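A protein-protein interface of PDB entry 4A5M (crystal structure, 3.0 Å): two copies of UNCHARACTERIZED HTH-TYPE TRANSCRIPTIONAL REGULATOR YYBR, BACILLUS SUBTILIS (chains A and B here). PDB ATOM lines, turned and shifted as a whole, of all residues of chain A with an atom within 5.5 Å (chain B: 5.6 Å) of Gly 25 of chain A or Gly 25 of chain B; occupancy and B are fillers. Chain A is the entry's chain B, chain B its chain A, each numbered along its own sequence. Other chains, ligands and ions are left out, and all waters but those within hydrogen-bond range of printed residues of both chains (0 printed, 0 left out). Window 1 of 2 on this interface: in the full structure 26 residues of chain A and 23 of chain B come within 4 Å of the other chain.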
ATOM      1  N   LEU A  20      34.610 -29.300  -7.977  1.00  0.00           N
ATOM      2  CA  LEU A  20      33.560 -28.875  -8.902  1.00  0.00           C
ATOM      3  C   LEU A  20      33.586 -29.660 -10.201  1.00  0.00           C
ATOM      4  O   LEU A  20      32.526 -29.981 -10.723  1.00  0.00           O
ATOM      5  CB  LEU A  20      33.613 -27.371  -9.176  1.00  0.00           C
ATOM      6  CG  LEU A  20      32.736 -26.596  -8.185  1.00  0.00           C
ATOM      7  CD1 LEU A  20      32.994 -25.102  -8.270  1.00  0.00           C
ATOM      8  CD2 LEU A  20      31.253 -26.898  -8.386  1.00  0.00           C
ATOM      9  N   ILE A  23      31.993 -33.042  -8.952  1.00  0.00           N
ATOM     10  CA  ILE A  23      30.604 -32.977  -8.472  1.00  0.00           C
ATOM     11  C   ILE A  23      29.775 -31.757  -8.932  1.00  0.00           C
ATOM     12  O   ILE A  23      28.539 -31.789  -8.897  1.00  0.00           O
ATOM     13  CB  ILE A  23      30.607 -33.059  -6.925  1.00  0.00           C
ATOM     14  CG1 ILE A  23      29.293 -33.624  -6.445  1.00  0.00           C
ATOM     15  CG2 ILE A  23      30.852 -31.690  -6.308  1.00  0.00           C
ATOM     16  CD1 ILE A  23      28.997 -35.036  -6.893  1.00  0.00           C
ATOM     17  N   GLY A  24      30.443 -30.708  -9.401  1.00  0.00           N
ATOM     18  CA  GLY A  24      29.746 -29.555  -9.931  1.00  0.00           C
ATOM     19  C   GLY A  24      28.998 -29.932 -11.183  1.00  0.00           C
ATOM     20  O   GLY A  24      28.958 -31.103 -11.581  1.00  0.00           O
ATOM     21  N   GLY A  25      28.369 -28.946 -11.797  1.00  0.00           N
ATOM     22  CA  GLY A  25      27.628 -29.192 -13.008  1.00  0.00           C
ATOM     23  C   GLY A  25      26.201 -29.526 -12.645  1.00  0.00           C
ATOM     24  O   GLY A  25      25.933 -30.138 -11.599  1.00  0.00           O
ATOM     25  N   LYS A  26      25.302 -29.145 -13.546  1.00  0.00           N
ATOM     26  CA  LYS A  26      23.875 -29.193 -13.329  1.00  0.00           C
ATOM     27  C   LYS A  26      23.398 -30.469 -12.658  1.00  0.00           C
ATOM     28  O   LYS A  26      22.686 -30.392 -11.665  1.00  0.00           O
ATOM     29  CB  LYS A  26      23.114 -29.062 -14.652  1.00  0.00           C
ATOM     30  CG  LYS A  26      21.625 -28.791 -14.500  1.00  0.00           C
ATOM     31  CD  LYS A  26      21.051 -28.035 -15.699  1.00  0.00           C
ATOM     32  CE  LYS A  26      19.685 -27.403 -15.380  1.00  0.00           C
ATOM     33  NZ  LYS A  26      18.999 -26.632 -16.462  1.00  0.00           N
ATOM     34  N   TRP A  27      23.792 -31.630 -13.188  1.00  0.00           N
ATOM     35  CA  TRP A  27      23.120 -32.897 -12.848  1.00  0.00           C
ATOM     36  C   TRP A  27      23.842 -33.755 -11.847  1.00  0.00           C
ATOM     37  O   TRP A  27      23.227 -34.337 -10.940  1.00  0.00           O
ATOM     38  CB  TRP A  27      22.848 -33.713 -14.105  1.00  0.00           C
ATOM     39  CG  TRP A  27      22.185 -32.911 -15.200  1.00  0.00           C
ATOM     40  CD1 TRP A  27      22.746 -32.436 -16.386  1.00  0.00           C
ATOM     41  CD2 TRP A  27      20.798 -32.439 -15.219  1.00  0.00           C
ATOM     42  NE1 TRP A  27      21.820 -31.738 -17.122  1.00  0.00           N
ATOM     43  CE2 TRP A  27      20.632 -31.702 -16.477  1.00  0.00           C
ATOM     44  CE3 TRP A  27      19.709 -32.552 -14.351  1.00  0.00           C
ATOM     45  CZ2 TRP A  27      19.425 -31.119 -16.827  1.00  0.00           C
ATOM     46  CZ3 TRP A  27      18.497 -31.951 -14.715  1.00  0.00           C
ATOM     47  CH2 TRP A  27      18.364 -31.255 -15.926  1.00  0.00           C
ATOM     48  N   LYS A  28      25.160 -33.814 -11.960  1.00  0.00           N
ATOM     49  CA  LYS A  28      25.908 -34.721 -11.124  1.00  0.00           C
ATOM     50  C   LYS A  28      25.350 -34.723  -9.681  1.00  0.00           C
ATOM     51  O   LYS A  28      25.018 -35.781  -9.120  1.00  0.00           O
ATOM     52  CB  LYS A  28      27.403 -34.399 -11.200  1.00  0.00           C
ATOM     53  CG  LYS A  28      27.983 -34.789 -12.550  1.00  0.00           C
ATOM     54  CD  LYS A  28      29.498 -34.902 -12.575  1.00  0.00           C
ATOM     55  CE  LYS A  28      30.003 -34.995 -14.015  1.00  0.00           C
ATOM     56  NZ  LYS A  28      31.447 -34.658 -14.147  1.00  0.00           N
ATOM     57  N   GLY A  29      25.163 -33.543  -9.108  1.00  0.00           N
ATOM     58  CA  GLY A  29      24.558 -33.462  -7.793  1.00  0.00           C
ATOM     59  C   GLY A  29      23.206 -34.154  -7.663  1.00  0.00           C
ATOM     60  O   GLY A  29      22.976 -34.882  -6.688  1.00  0.00           O
ATOM     61  N   LEU B  20      22.377 -26.059  -7.150  1.00  0.00           N
ATOM     62  CA  LEU B  20      23.439 -26.303  -8.130  1.00  0.00           C
ATOM     63  C   LEU B  20      23.388 -25.292  -9.262  1.00  0.00           C
ATOM     64  O   LEU B  20      24.433 -24.888  -9.753  1.00  0.00           O
ATOM     65  CB  LEU B  20      23.399 -27.746  -8.649  1.00  0.00           C
ATOM     66  CG  LEU B  20      24.114 -28.783  -7.767  1.00  0.00           C
ATOM     67  CD1 LEU B  20      23.272 -30.036  -7.669  1.00  0.00           C
ATOM     68  CD2 LEU B  20      25.596 -29.029  -8.123  1.00  0.00           C
ATOM     69  N   ILE B  23      24.937 -22.154  -7.445  1.00  0.00           N
ATOM     70  CA  ILE B  23      26.340 -22.289  -7.055  1.00  0.00           C
ATOM     71  C   ILE B  23      27.190 -23.389  -7.766  1.00  0.00           C
ATOM     72  O   ILE B  23      28.427 -23.365  -7.755  1.00  0.00           O
ATOM     73  CB  ILE B  23      26.363 -22.560  -5.578  1.00  0.00           C
ATOM     74  CG1 ILE B  23      27.732 -22.104  -5.041  1.00  0.00           C
ATOM     75  CG2 ILE B  23      26.020 -24.068  -5.395  1.00  0.00           C
ATOM     76  CD1 ILE B  23      28.172 -20.766  -5.527  1.00  0.00           C
ATOM     77  N   GLY B  24      26.534 -24.338  -8.409  1.00  0.00           N
ATOM     78  CA  GLY B  24      27.240 -25.385  -9.150  1.00  0.00           C
ATOM     79  C   GLY B  24      27.960 -24.755 -10.307  1.00  0.00           C
ATOM     80  O   GLY B  24      27.950 -23.540 -10.478  1.00  0.00           O
ATOM     81  N   GLY B  25      28.582 -25.572 -11.121  1.00  0.00           N
ATOM     82  CA  GLY B  25      29.250 -25.043 -12.292  1.00  0.00           C
ATOM     83  C   GLY B  25      30.670 -24.715 -11.934  1.00  0.00           C
ATOM     84  O   GLY B  25      30.994 -24.405 -10.794  1.00  0.00           O
ATOM     85  N   LYS B  26      31.526 -24.867 -12.924  1.00  0.00           N
ATOM     86  CA  LYS B  26      32.984 -24.805 -12.755  1.00  0.00           C
ATOM     87  C   LYS B  26      33.489 -23.758 -11.800  1.00  0.00           C
ATOM     88  O   LYS B  26      34.229 -24.060 -10.870  1.00  0.00           O
ATOM     89  CB  LYS B  26      33.512 -24.378 -14.090  1.00  0.00           C
ATOM     90  CG  LYS B  26      32.935 -25.194 -15.196  1.00  0.00           C
ATOM     91  CD  LYS B  26      31.954 -24.373 -16.005  1.00  0.00           C
ATOM     92  CE  LYS B  26      31.015 -25.257 -16.790  1.00  0.00           C
ATOM     93  NZ  LYS B  26      30.021 -24.419 -17.531  1.00  0.00           N
ATOM     94  N   TRP B  27      33.090 -22.520 -12.079  1.00  0.00           N
ATOM     95  CA  TRP B  27      33.773 -21.366 -11.519  1.00  0.00           C
ATOM     96  C   TRP B  27      33.040 -20.751 -10.357  1.00  0.00           C
ATOM     97  O   TRP B  27      33.653 -20.340  -9.361  1.00  0.00           O
ATOM     98  CB  TRP B  27      34.003 -20.325 -12.584  1.00  0.00           C
ATOM     99  CG  TRP B  27      34.692 -20.851 -13.813  1.00  0.00           C
ATOM    100  CD1 TRP B  27      34.137 -21.078 -15.070  1.00  0.00           C
ATOM    101  CD2 TRP B  27      36.111 -21.216 -13.951  1.00  0.00           C
ATOM    102  NE1 TRP B  27      35.091 -21.540 -15.939  1.00  0.00           N
ATOM    103  CE2 TRP B  27      36.289 -21.651 -15.326  1.00  0.00           C
ATOM    104  CE3 TRP B  27      37.197 -21.229 -13.101  1.00  0.00           C
ATOM    105  CZ2 TRP B  27      37.509 -22.080 -15.809  1.00  0.00           C
ATOM    106  CZ3 TRP B  27      38.428 -21.652 -13.597  1.00  0.00           C
ATOM    107  CH2 TRP B  27      38.576 -22.073 -14.925  1.00  0.00           C
ATOM    108  N   LYS B  28      31.717 -20.705 -10.443  1.00  0.00           N
ATOM    109  CA  LYS B  28      30.969 -20.000  -9.440  1.00  0.00           C
ATOM    110  C   LYS B  28      31.585 -20.260  -8.055  1.00  0.00           C
ATOM    111  O   LYS B  28      31.862 -19.328  -7.286  1.00  0.00           O
ATOM    112  CB  LYS B  28      29.488 -20.351  -9.530  1.00  0.00           C
ATOM    113  CG  LYS B  28      28.858 -19.749 -10.782  1.00  0.00           C
ATOM    114  CD  LYS B  28      27.339 -19.688 -10.773  1.00  0.00           C
ATOM    115  CE  LYS B  28      26.847 -19.372 -12.154  1.00  0.00           C
ATOM    116  NZ  LYS B  28      25.469 -19.908 -12.328  1.00  0.00           N
ATOM    117  N   GLY B  29      31.834 -21.520  -7.743  1.00  0.00           N
ATOM    118  CA  GLY B  29      32.434 -21.827  -6.454  1.00  0.00           C
ATOM    119  C   GLY B  29      33.733 -21.087  -6.213  1.00  0.00           C
ATOM    120  O   GLY B  29      33.958 -20.599  -5.120  1.00  0.00           O
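Leu 20 of chain A touches Gly 25 of chain B, and with the chains exchanged Gly 25 of chain A touches Leu 20 of chain B.
Leu 20 of chain A touches Lys 26 of chain B, but with the chains exchanged Lys 26 of chain A does not touch Leu 20 of chain B (4.1 Å).
Leu 20 of chain A touches Gly 29 of chain B, and with the chains exchanged Gly 29 of chain A touches Leu 20 of chain B.
Gly 25 of chain B touches its own counterpart, Gly 25 of chain A.
Leu 20 of chain A touches Gly 25 of chain B (CD1 to O, 3.3 Å).
Leu 20 of chain A touches Lys 26 of chain B.
Leu 20 of chain A touches Gly 29 of chain B (CD1 to CA, 3.8 Å).
CD2 of Leu 20 of chain B touches O of Gly 25 of chain A, at 3.7 Å.
Leu 20 of chain B touches Gly 29 of chain A.
Printed residues of chain B that touch a printed residue of chain A: Leu 20, Gly 25, Lys 26 and Gly 29.
Hydrophobic or aromatic side chains of chain B within 4 Å of the printed part of chain A: Leu 20.
Of the 8 printed residues of chain A, 3 touch a printed residue of chain B.
Among the printed residues, 6 pairs touch across the chains.
The backbone NH of Gly 25 of chain A lies close to the backbone NH of Gly 25 of chain B (3.4 Å).
Gly 25 of chain A touches just these residues of chain B: Leu 20 (3.7 Å) and Gly 25 (3.4 Å).
Printed residues of chain A within 4 Å of Leu 20 of chain B: Gly 25 and Gly 29.
Gly 25 of chain B touches just these residues of chain A: Leu 20 and Gly 25.
Printed residues of chain A within 4 Å of Lys 26 of chain B: Leu 20.
Printed residues of chain A within 4 Å of Gly 29 of chain B: Leu 20.
The nearest residue of chain A that does not touch Gly 25 of chain B is Gly 24 of chain A (4.3 Å).
The nearest printed residue of chain B that does not touch Gly 29 of chain A is Gly 24 of chain B (8.4 Å).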
